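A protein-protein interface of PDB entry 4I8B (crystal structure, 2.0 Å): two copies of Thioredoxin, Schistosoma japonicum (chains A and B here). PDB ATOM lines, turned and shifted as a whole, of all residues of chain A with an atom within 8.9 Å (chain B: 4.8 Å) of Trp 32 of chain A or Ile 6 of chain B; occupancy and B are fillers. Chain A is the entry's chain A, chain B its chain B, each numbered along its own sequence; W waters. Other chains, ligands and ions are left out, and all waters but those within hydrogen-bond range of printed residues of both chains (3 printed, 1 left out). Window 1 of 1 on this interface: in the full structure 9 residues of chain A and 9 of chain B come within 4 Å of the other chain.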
ATOM      1  N   PHE A  28       0.297 -21.363  23.287  1.00  0.00           N
ATOM      2  CA  PHE A  28       1.346 -22.381  23.232  1.00  0.00           C
ATOM      3  C   PHE A  28       2.699 -21.694  23.085  1.00  0.00           C
ATOM      4  O   PHE A  28       2.914 -20.936  22.138  1.00  0.00           O
ATOM      5  CB  PHE A  28       1.160 -23.305  22.030  1.00  0.00           C
ATOM      6  CG  PHE A  28       0.038 -24.283  22.191  1.00  0.00           C
ATOM      7  CD1 PHE A  28      -1.260 -23.916  21.906  1.00  0.00           C
ATOM      8  CD2 PHE A  28       0.293 -25.584  22.622  1.00  0.00           C
ATOM      9  CE1 PHE A  28      -2.297 -24.830  22.052  1.00  0.00           C
ATOM     10  CE2 PHE A  28      -0.731 -26.489  22.772  1.00  0.00           C
ATOM     11  CZ  PHE A  28      -2.026 -26.113  22.485  1.00  0.00           C
ATOM     12  N   PHE A  29       3.606 -21.983  24.010  1.00  0.00           N
ATOM     13  CA  PHE A  29       4.887 -21.290  24.081  1.00  0.00           C
ATOM     14  C   PHE A  29       6.026 -22.285  24.287  1.00  0.00           C
ATOM     15  O   PHE A  29       5.799 -23.468  24.565  1.00  0.00           O
ATOM     16  CB  PHE A  29       4.854 -20.234  25.210  1.00  0.00           C
ATOM     17  CG  PHE A  29       4.997 -20.814  26.604  1.00  0.00           C
ATOM     18  CD1 PHE A  29       3.884 -21.229  27.316  1.00  0.00           C
ATOM     19  CD2 PHE A  29       6.243 -20.943  27.193  1.00  0.00           C
ATOM     20  CE1 PHE A  29       4.009 -21.776  28.575  1.00  0.00           C
ATOM     21  CE2 PHE A  29       6.375 -21.485  28.459  1.00  0.00           C
ATOM     22  CZ  PHE A  29       5.249 -21.894  29.158  1.00  0.00           C
ATOM     23  N   ALA A  30       7.261 -21.827  24.139  1.00  0.00           N
ATOM     24  CA  ALA A  30       8.404 -22.682  24.469  1.00  0.00           C
ATOM     25  C   ALA A  30       9.333 -21.893  25.382  1.00  0.00           C
ATOM     26  O   ALA A  30       9.348 -20.673  25.307  1.00  0.00           O
ATOM     27  CB  ALA A  30       9.138 -23.096  23.206  1.00  0.00           C
ATOM     28  N   THR A  31      10.085 -22.578  26.247  1.00  0.00           N
ATOM     29  CA  THR A  31      10.950 -21.888  27.219  1.00  0.00           C
ATOM     30  C   THR A  31      12.067 -21.056  26.557  1.00  0.00           C
ATOM     31  O   THR A  31      12.472 -19.997  27.071  1.00  0.00           O
ATOM     32  CB  THR A  31      11.547 -22.860  28.259  1.00  0.00           C
ATOM     33  OG1 THR A  31      12.187 -23.949  27.594  1.00  0.00           O
ATOM     34  CG2 THR A  31      10.441 -23.432  29.177  1.00  0.00           C
ATOM     35  N   TRP A  32      12.540 -21.522  25.405  1.00  0.00           N
ATOM     36  CA  TRP A  32      13.621 -20.846  24.680  1.00  0.00           C
ATOM     37  C   TRP A  32      13.153 -19.668  23.800  1.00  0.00           C
ATOM     38  O   TRP A  32      13.968 -19.058  23.089  1.00  0.00           O
ATOM     39  CB  TRP A  32      14.372 -21.868  23.814  1.00  0.00           C
ATOM     40  CG  TRP A  32      13.439 -22.754  23.019  1.00  0.00           C
ATOM     41  CD1 TRP A  32      13.073 -24.033  23.319  1.00  0.00           C
ATOM     42  CD2 TRP A  32      12.746 -22.412  21.810  1.00  0.00           C
ATOM     43  NE1 TRP A  32      12.205 -24.517  22.367  1.00  0.00           N
ATOM     44  CE2 TRP A  32      11.991 -23.544  21.428  1.00  0.00           C
ATOM     45  CE3 TRP A  32      12.701 -21.265  21.007  1.00  0.00           C
ATOM     46  CZ2 TRP A  32      11.196 -23.561  20.283  1.00  0.00           C
ATOM     47  CZ3 TRP A  32      11.910 -21.283  19.863  1.00  0.00           C
ATOM     48  CH2 TRP A  32      11.166 -22.423  19.517  1.00  0.00           C
ATOM     49  N   CYS A  33      11.859 -19.361  23.835  1.00  0.00           N
ATOM     50  CA  CYS A  33      11.257 -18.422  22.875  1.00  0.00           C
ATOM     51  C   CYS A  33      11.151 -17.005  23.447  1.00  0.00           C
ATOM     52  O   CYS A  33      10.429 -16.781  24.420  1.00  0.00           O
ATOM     53  CB  CYS A  33       9.876 -18.956  22.433  1.00  0.00           C
ATOM     54  SG  CYS A  33       8.728 -17.826  21.556  1.00  0.00           S
ATOM     55  N   GLY A  34      11.871 -16.059  22.844  1.00  0.00           N
ATOM     56  CA  GLY A  34      11.939 -14.687  23.334  1.00  0.00           C
ATOM     57  C   GLY A  34      10.652 -13.904  23.145  1.00  0.00           C
ATOM     58  O   GLY A  34      10.173 -13.236  24.063  1.00  0.00           O
ATOM     59  N   PRO A  35      10.086 -13.958  21.936  1.00  0.00           N
ATOM     60  CA  PRO A  35       8.811 -13.280  21.713  1.00  0.00           C
ATOM     61  C   PRO A  35       7.689 -13.827  22.591  1.00  0.00           C
ATOM     62  O   PRO A  35       6.802 -13.054  22.947  1.00  0.00           O
ATOM     63  CB  PRO A  35       8.537 -13.559  20.235  1.00  0.00           C
ATOM     64  CG  PRO A  35       9.938 -13.579  19.645  1.00  0.00           C
ATOM     65  CD  PRO A  35      10.707 -14.377  20.667  1.00  0.00           C
ATOM     66  N   CYS A  36       7.713 -15.113  22.941  1.00  0.00           N
ATOM     67  CA  CYS A  36       6.707 -15.643  23.878  1.00  0.00           C
ATOM     68  C   CYS A  36       6.797 -14.891  25.199  1.00  0.00           C
ATOM     69  O   CYS A  36       5.781 -14.444  25.760  1.00  0.00           O
ATOM     70  CB  CYS A  36       6.900 -17.149  24.118  1.00  0.00           C
ATOM     71  SG  CYS A  36       6.914 -18.139  22.607  1.00  0.00           S
ATOM     72  N   LYS A  37       8.021 -14.744  25.700  1.00  0.00           N
ATOM     73  CA  LYS A  37       8.207 -14.041  26.965  1.00  0.00           C
ATOM     74  C   LYS A  37       7.798 -12.574  26.879  1.00  0.00           C
ATOM     75  O   LYS A  37       7.286 -12.013  27.847  1.00  0.00           O
ATOM     76  CB  LYS A  37       9.665 -14.171  27.446  1.00  0.00           C
ATOM     77  CG  LYS A  37      10.042 -15.635  27.803  1.00  0.00           C
ATOM     78  CD  LYS A  37      11.501 -15.756  28.221  1.00  0.00           C
ATOM     79  CE  LYS A  37      11.922 -17.238  28.220  1.00  0.00           C
ATOM     80  NZ  LYS A  37      13.272 -17.362  28.822  1.00  0.00           N
ATOM     81  N   ASP A  58       3.209 -25.014  27.792  1.00  0.00           N
ATOM     82  CA  ASP A  58       4.577 -25.255  27.325  1.00  0.00           C
ATOM     83  C   ASP A  58       4.587 -26.431  26.343  1.00  0.00           C
ATOM     84  O   ASP A  58       4.254 -27.571  26.716  1.00  0.00           O
ATOM     85  CB  ASP A  58       5.436 -25.570  28.552  1.00  0.00           C
ATOM     86  CG  ASP A  58       6.903 -25.826  28.220  1.00  0.00           C
ATOM     87  OD1 ASP A  58       7.242 -26.240  27.082  1.00  0.00           O
ATOM     88  OD2 ASP A  58       7.720 -25.618  29.138  1.00  0.00           O
ATOM     89  N   VAL A  59       4.969 -26.169  25.093  1.00  0.00           N
ATOM     90  CA  VAL A  59       4.939 -27.207  24.054  1.00  0.00           C
ATOM     91  C   VAL A  59       5.815 -28.405  24.361  1.00  0.00           C
ATOM     92  O   VAL A  59       5.550 -29.501  23.864  1.00  0.00           O
ATOM     93  CB  VAL A  59       5.301 -26.682  22.640  1.00  0.00           C
ATOM     94  CG1 VAL A  59       4.291 -25.657  22.176  1.00  0.00           C
ATOM     95  CG2 VAL A  59       6.727 -26.127  22.604  1.00  0.00           C
ATOM     96  N   ASP A  60       6.847 -28.220  25.182  1.00  0.00           N
ATOM     97  CA  ASP A  60       7.709 -29.352  25.543  1.00  0.00           C
ATOM     98  C   ASP A  60       7.075 -30.246  26.610  1.00  0.00           C
ATOM     99  O   ASP A  60       7.472 -31.399  26.809  1.00  0.00           O
ATOM    100  CB  ASP A  60       9.074 -28.856  26.025  1.00  0.00           C
ATOM    101  CG  ASP A  60       9.907 -28.293  24.896  1.00  0.00           C
ATOM    102  OD1 ASP A  60       9.717 -28.779  23.761  1.00  0.00           O
ATOM    103  OD2 ASP A  60      10.728 -27.370  25.138  1.00  0.00           O
ATOM    104  N   SER A  72       3.549 -25.366  15.386  1.00  0.00           N
ATOM    105  CA  SER A  72       4.936 -25.565  14.965  1.00  0.00           C
ATOM    106  C   SER A  72       5.861 -24.357  15.195  1.00  0.00           C
ATOM    107  O   SER A  72       7.078 -24.512  15.278  1.00  0.00           O
ATOM    108  CB  SER A  72       5.015 -26.065  13.514  1.00  0.00           C
ATOM    109  OG  SER A  72       4.500 -25.099  12.619  1.00  0.00           O
ATOM    110  N   ALA A  73       5.280 -23.170  15.303  1.00  0.00           N
ATOM    111  CA  ALA A  73       6.044 -21.934  15.528  1.00  0.00           C
ATOM    112  C   ALA A  73       5.530 -21.289  16.809  1.00  0.00           C
ATOM    113  O   ALA A  73       4.352 -21.423  17.138  1.00  0.00           O
ATOM    114  CB  ALA A  73       5.884 -20.993  14.371  1.00  0.00           C
ATOM    115  N   MET A  74       6.412 -20.598  17.527  1.00  0.00           N
ATOM    116  CA  MET A  74       6.110 -20.115  18.889  1.00  0.00           C
ATOM    117  C   MET A  74       6.144 -18.597  18.914  1.00  0.00           C
ATOM    118  O   MET A  74       6.999 -17.998  18.265  1.00  0.00           O
ATOM    119  CB  MET A  74       7.199 -20.624  19.831  1.00  0.00           C
ATOM    120  CG  MET A  74       6.722 -21.501  20.949  1.00  0.00           C
ATOM    121  SD  MET A  74       5.971 -23.009  20.360  1.00  0.00           S
ATOM    122  CE  MET A  74       7.173 -23.545  19.177  1.00  0.00           C
ATOM    123  N   PRO A  75       5.196 -17.960  19.622  1.00  0.00           N
ATOM    124  CA  PRO A  75       4.026 -18.580  20.263  1.00  0.00           C
ATOM    125  C   PRO A  75       2.966 -18.842  19.200  1.00  0.00           C
ATOM    126  O   PRO A  75       2.994 -18.191  18.153  1.00  0.00           O
ATOM    127  CB  PRO A  75       3.531 -17.482  21.210  1.00  0.00           C
ATOM    128  CG  PRO A  75       3.871 -16.202  20.456  1.00  0.00           C
ATOM    129  CD  PRO A  75       5.235 -16.500  19.840  1.00  0.00           C
ATOM    130  N   LEU B   4      10.532 -28.566  14.781  1.00  0.00           N
ATOM    131  CA  LEU B   4      10.372 -27.238  15.335  1.00  0.00           C
ATOM    132  C   LEU B   4      10.752 -26.152  14.323  1.00  0.00           C
ATOM    133  O   LEU B   4      11.703 -26.307  13.558  1.00  0.00           O
ATOM    134  CB  LEU B   4      11.275 -27.130  16.548  1.00  0.00           C
ATOM    135  CG  LEU B   4      11.221 -25.832  17.326  1.00  0.00           C
ATOM    136  CD1 LEU B   4       9.782 -25.542  17.775  1.00  0.00           C
ATOM    137  CD2 LEU B   4      12.173 -25.970  18.494  1.00  0.00           C
ATOM    138  N   HIS B   5       9.989 -25.066  14.313  1.00  0.00           N
ATOM    139  CA  HIS B   5      10.287 -23.910  13.486  1.00  0.00           C
ATOM    140  C   HIS B   5      10.834 -22.806  14.394  1.00  0.00           C
ATOM    141  O   HIS B   5      10.119 -22.297  15.255  1.00  0.00           O
ATOM    142  CB  HIS B   5       9.010 -23.447  12.781  1.00  0.00           C
ATOM    143  CG  HIS B   5       9.251 -22.588  11.580  1.00  0.00           C
ATOM    144  ND1 HIS B   5       9.916 -21.381  11.646  1.00  0.00           N
ATOM    145  CD2 HIS B   5       8.908 -22.756  10.281  1.00  0.00           C
ATOM    146  CE1 HIS B   5       9.977 -20.846  10.441  1.00  0.00           C
ATOM    147  NE2 HIS B   5       9.371 -21.660   9.593  1.00  0.00           N
ATOM    148  N   ILE B   6      12.108 -22.458  14.230  1.00  0.00           N
ATOM    149  CA  ILE B   6      12.727 -21.417  15.050  1.00  0.00           C
ATOM    150  C   ILE B   6      12.936 -20.186  14.173  1.00  0.00           C
ATOM    151  O   ILE B   6      13.390 -20.300  13.033  1.00  0.00           O
ATOM    152  CB  ILE B   6      14.048 -21.903  15.683  1.00  0.00           C
ATOM    153  CG1 ILE B   6      13.792 -23.093  16.613  1.00  0.00           C
ATOM    154  CG2 ILE B   6      14.778 -20.752  16.433  1.00  0.00           C
ATOM    155  CD1 ILE B   6      15.055 -23.664  17.230  1.00  0.00           C
ATOM    156  N   GLU B   7      12.610 -19.009  14.695  1.00  0.00           N
ATOM    157  CA  GLU B   7      12.389 -17.848  13.828  1.00  0.00           C
ATOM    158  C   GLU B   7      13.236 -16.608  14.098  1.00  0.00           C
ATOM    159  O   GLU B   7      13.141 -15.627  13.356  1.00  0.00           O
ATOM    160  CB  GLU B   7      10.905 -17.461  13.846  1.00  0.00           C
ATOM    161  CG  GLU B   7       9.984 -18.493  13.212  1.00  0.00           C
ATOM    162  CD  GLU B   7       8.538 -18.041  13.227  1.00  0.00           C
ATOM    163  OE1 GLU B   7       8.044 -17.682  14.319  1.00  0.00           O
ATOM    164  OE2 GLU B   7       7.902 -18.031  12.152  1.00  0.00           O
ATOM    165  N   THR B   8      14.056 -16.636  15.143  1.00  0.00           N
ATOM    166  CA  THR B   8      15.023 -15.570  15.378  1.00  0.00           C
ATOM    167  C   THR B   8      16.352 -16.167  15.833  1.00  0.00           C
ATOM    168  O   THR B   8      16.389 -17.300  16.309  1.00  0.00           O
ATOM    169  CB  THR B   8      14.549 -14.576  16.470  1.00  0.00           C
ATOM    170  OG1 THR B   8      14.930 -15.061  17.761  1.00  0.00           O
ATOM    171  CG2 THR B   8      13.040 -14.377  16.425  1.00  0.00           C
ATOM    172  N   ASP B  11      16.427 -16.877  19.717  1.00  0.00           N
ATOM    173  CA  ASP B  11      15.680 -18.098  20.007  1.00  0.00           C
ATOM    174  C   ASP B  11      16.545 -19.323  19.687  1.00  0.00           C
ATOM    175  O   ASP B  11      16.603 -20.282  20.469  1.00  0.00           O
ATOM    176  CB  ASP B  11      14.371 -18.150  19.216  1.00  0.00           C
ATOM    177  CG  ASP B  11      13.309 -17.227  19.787  1.00  0.00           C
ATOM    178  OD1 ASP B  11      13.636 -16.438  20.693  1.00  0.00           O
ATOM    179  OD2 ASP B  11      12.153 -17.289  19.321  1.00  0.00           O
ATOM    180  N   PHE B  12      17.219 -19.291  18.548  1.00  0.00           N
ATOM    181  CA  PHE B  12      18.098 -20.399  18.202  1.00  0.00           C
ATOM    182  C   PHE B  12      19.181 -20.580  19.259  1.00  0.00           C
ATOM    183  O   PHE B  12      19.415 -21.697  19.731  1.00  0.00           O
ATOM    184  CB  PHE B  12      18.743 -20.218  16.833  1.00  0.00           C
ATOM    185  CG  PHE B  12      19.474 -21.441  16.372  1.00  0.00           C
ATOM    186  CD1 PHE B  12      18.811 -22.431  15.663  1.00  0.00           C
ATOM    187  CD2 PHE B  12      20.815 -21.630  16.693  1.00  0.00           C
ATOM    188  CE1 PHE B  12      19.484 -23.577  15.254  1.00  0.00           C
ATOM    189  CE2 PHE B  12      21.491 -22.765  16.285  1.00  0.00           C
ATOM    190  CZ  PHE B  12      20.824 -23.740  15.565  1.00  0.00           C
ATOM    191  N   SER B  14      19.093 -19.655  22.371  1.00  0.00           N
ATOM    192  CA  SER B  14      18.470 -20.156  23.599  1.00  0.00           C
ATOM    193  C   SER B  14      18.138 -21.643  23.475  1.00  0.00           C
ATOM    194  O   SER B  14      18.404 -22.435  24.377  1.00  0.00           O
ATOM    195  CB  SER B  14      17.203 -19.365  23.933  1.00  0.00           C
ATOM    196  OG  SER B  14      17.470 -17.979  24.070  1.00  0.00           O
ATOM    197  N   PHE B  15      17.545 -22.021  22.346  1.00  0.00           N
ATOM    198  CA  PHE B  15      17.231 -23.428  22.092  1.00  0.00           C
ATOM    199  C   PHE B  15      18.483 -24.300  22.238  1.00  0.00           C
ATOM    200  O   PHE B  15      18.469 -25.346  22.905  1.00  0.00           O
ATOM    201  CB  PHE B  15      16.632 -23.604  20.685  1.00  0.00           C
ATOM    202  CG  PHE B  15      16.410 -25.035  20.300  1.00  0.00           C
ATOM    203  CD1 PHE B  15      15.339 -25.742  20.814  1.00  0.00           C
ATOM    204  CD2 PHE B  15      17.269 -25.674  19.419  1.00  0.00           C
ATOM    205  CE1 PHE B  15      15.127 -27.064  20.464  1.00  0.00           C
ATOM    206  CE2 PHE B  15      17.062 -26.993  19.066  1.00  0.00           C
ATOM    207  CZ  PHE B  15      15.990 -27.691  19.599  1.00  0.00           C
ATOM    208  N   GLU B  18      19.517 -24.908  25.798  1.00  0.00           N
ATOM    209  CA  GLU B  18      18.657 -25.848  26.523  1.00  0.00           C
ATOM    210  C   GLU B  18      18.923 -27.283  26.142  1.00  0.00           C
ATOM    211  O   GLU B  18      18.514 -28.207  26.845  1.00  0.00           O
ATOM    212  CB  GLU B  18      17.194 -25.563  26.234  1.00  0.00           C
ATOM    213  CG  GLU B  18      16.659 -24.354  26.936  1.00  0.00           C
ATOM    214  CD  GLU B  18      15.163 -24.235  26.765  1.00  0.00           C
ATOM    215  OE1 GLU B  18      14.540 -25.196  26.258  1.00  0.00           O
ATOM    216  OE2 GLU B  18      14.615 -23.182  27.125  1.00  0.00           O
ATOM    217  N   VAL B  55      14.930 -29.404  13.462  1.00  0.00           N
ATOM    218  CA  VAL B  55      14.551 -27.998  13.478  1.00  0.00           C
ATOM    219  C   VAL B  55      14.592 -27.397  12.076  1.00  0.00           C
ATOM    220  O   VAL B  55      15.421 -27.783  11.252  1.00  0.00           O
ATOM    221  CB  VAL B  55      15.501 -27.193  14.395  1.00  0.00           C
ATOM    222  CG1 VAL B  55      15.282 -25.694  14.219  1.00  0.00           C
ATOM    223  CG2 VAL B  55      15.333 -27.614  15.844  1.00  0.00           C
ATOM    224  N   LYS B  56      13.684 -26.464  11.803  1.00  0.00           N
ATOM    225  CA  LYS B  56      13.660 -25.766  10.517  1.00  0.00           C
ATOM    226  C   LYS B  56      13.921 -24.291  10.751  1.00  0.00           C
ATOM    227  O   LYS B  56      13.311 -23.678  11.634  1.00  0.00           O
ATOM    228  CB  LYS B  56      12.300 -25.934   9.834  1.00  0.00           C
ATOM    229  CG  LYS B  56      12.096 -27.299   9.212  1.00  0.00           C
ATOM    230  CD  LYS B  56      10.671 -27.481   8.714  1.00  0.00           C
ATOM    231  CE  LYS B  56      10.501 -26.955   7.296  1.00  0.00           C
ATOM    232  NZ  LYS B  56      11.342 -27.715   6.339  1.00  0.00           N
ATOM    233  N   VAL B  57      14.828 -23.726   9.969  1.00  0.00           N
ATOM    234  CA  VAL B  57      15.177 -22.319  10.106  1.00  0.00           C
ATOM    235  C   VAL B  57      15.233 -21.622   8.744  1.00  0.00           C
ATOM    236  O   VAL B  57      15.811 -22.138   7.789  1.00  0.00           O
ATOM    237  CB  VAL B  57      16.530 -22.168  10.822  1.00  0.00           C
ATOM    238  CG1 VAL B  57      17.139 -20.818  10.541  1.00  0.00           C
ATOM    239  CG2 VAL B  57      16.350 -22.381  12.311  1.00  0.00           C
ATOM    240  N   ASP B  58      14.613 -20.451   8.668  1.00  0.00           N
ATOM    241  CA  ASP B  58      14.605 -19.638   7.458  1.00  0.00           C
ATOM    242  C   ASP B  58      15.906 -18.845   7.385  1.00  0.00           C
ATOM    243  O   ASP B  58      16.137 -17.961   8.207  1.00  0.00           O
ATOM    244  CB  ASP B  58      13.402 -18.688   7.504  1.00  0.00           C
ATOM    245  CG  ASP B  58      13.139 -17.996   6.183  1.00  0.00           C
ATOM    246  OD1 ASP B  58      14.103 -17.528   5.546  1.00  0.00           O
ATOM    247  OD2 ASP B  58      11.959 -17.922   5.785  1.00  0.00           O
ATOM    248  N   LEU B  62      17.310 -15.759   9.943  1.00  0.00           N
ATOM    249  CA  LEU B  62      18.384 -16.049  10.890  1.00  0.00           C
ATOM    250  C   LEU B  62      19.764 -15.879  10.260  1.00  0.00           C
ATOM    251  O   LEU B  62      20.553 -16.825  10.185  1.00  0.00           O
ATOM    252  CB  LEU B  62      18.227 -17.455  11.491  1.00  0.00           C
ATOM    253  CG  LEU B  62      17.186 -17.651  12.612  1.00  0.00           C
ATOM    254  CD1 LEU B  62      15.766 -17.621  12.067  1.00  0.00           C
ATOM    255  CD2 LEU B  62      17.422 -18.957  13.373  1.00  0.00           C
HETATM  256  O   HOH W   1      15.474 -16.466  23.306  1.00  0.00           O
HETATM  257  O   HOH W   2      13.554 -27.572  24.806  1.00  0.00           O
HETATM  258  O   HOH W   3       9.241 -20.544  16.846  1.00  0.00           O
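The backbone NH (N) of Trp 32 of chain A lies within hydrogen-bond range of the side-chain carboxylate (OE2) of Glu 18 of chain B.
OG1 of Thr 31 of chain A is in hydrogen-bond range of OE2 of Glu 18 of chain B.
The backbone NH (N) of His 5 of chain B sits at hydrogen-bond distance from the backbone carbonyl oxygen (O) of Ser 72 of chain A, at 3.1 Å.
The backbone NH (N) of Gly 34 of chain A lies within hydrogen-bond range of the side-chain carboxylate (OD1) of Asp 11 of chain B (2.8 Å).
O of Leu 4 of chain B sits at hydrogen-bond distance from N of Lys 56 of chain B (2.7 Å).
O of Lys 56 of chain B lies within hydrogen-bond range of N of Ile 6 of chain B, at 3.1 Å.
SG of Cys 33 of chain A is disulfide-bonded to SG of Cys 36 of chain A, 2.1 Å away.
The side-chain hydroxyl (OG1) of Thr 8 of chain B is in hydrogen-bond range of the backbone NH (N) of Asp 11 of chain B, 3.1 Å away.
NZ of Lys 37 of chain A lies close to O of Thr 31 of chain A (3.3 Å).
Among the printed residues, merely in contact across the chains: Trp 32 of chain A with Leu 4 of chain B, Trp 32 of chain A with Ile 6 of chain B, Trp 32 of chain A with Asp 11 of chain B, Trp 32 of chain A with Ser 14 of chain B, Trp 32 of chain A with Phe 15 of chain B, Cys 33 of chain A with Asp 11 of chain B, Pro 35 of chain A with Asp 11 of chain B, Ser 72 of chain A with Leu 4 of chain B, Ala 73 of chain A with Glu 7 of chain B and Met 74 of chain A with Leu 4 of chain B.
Of the printed residues of chain B, Gly 34 of chain A touches Asp 11.
Printed residues of chain B within 4 Å of Pro 35 of chain A: Asp 11.
Printed residues of chain B within 4 Å of Ser 72 of chain A: Leu 4 (3.8 Å) and His 5 (3.1 Å).
Of the printed residues of chain A, Leu 4 of chain B touches Trp 32 (3.2 Å), Ser 72 (3.8 Å) and Met 74 (3.6 Å).
Of the printed residues of chain A, His 5 of chain B touches Ser 72 (3.1 Å).
Of chain A, only Trp 32 (3.97 Å) comes within 4 Å of Ile 6 of chain B.
The nearest printed residue of chain B that does not touch Trp 32 of chain A is His 5 of chain B (4.4 Å).
The nearest printed residue of chain A that does not touch His 5 of chain B is Ala 73 of chain A (4.1 Å).
Hydrophobic or aromatic side chains of chain B that line the printed part of chain A: Leu 4, His 5, Ile 6 and Phe 15.
Position printed for both chains: 58.
Water W3 lies within hydrogen-bond range of O of His 5 of chain B (2.5 Å) and N of Met 74 of chain A (2.9 Å).
Water W1 lies within hydrogen-bond range of OG of Ser 14 of chain B (2.6 Å), O of Trp 32 of chain A (3.0 Å) and OD1 of Asp 11 of chain B (3.2 Å).
Water W2 lies within hydrogen-bond range of the side-chain carboxylate of Asp 60 of chain A (2.9 Å) and the side-chain carboxylate of Glu 18 of chain B (3.0 Å).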
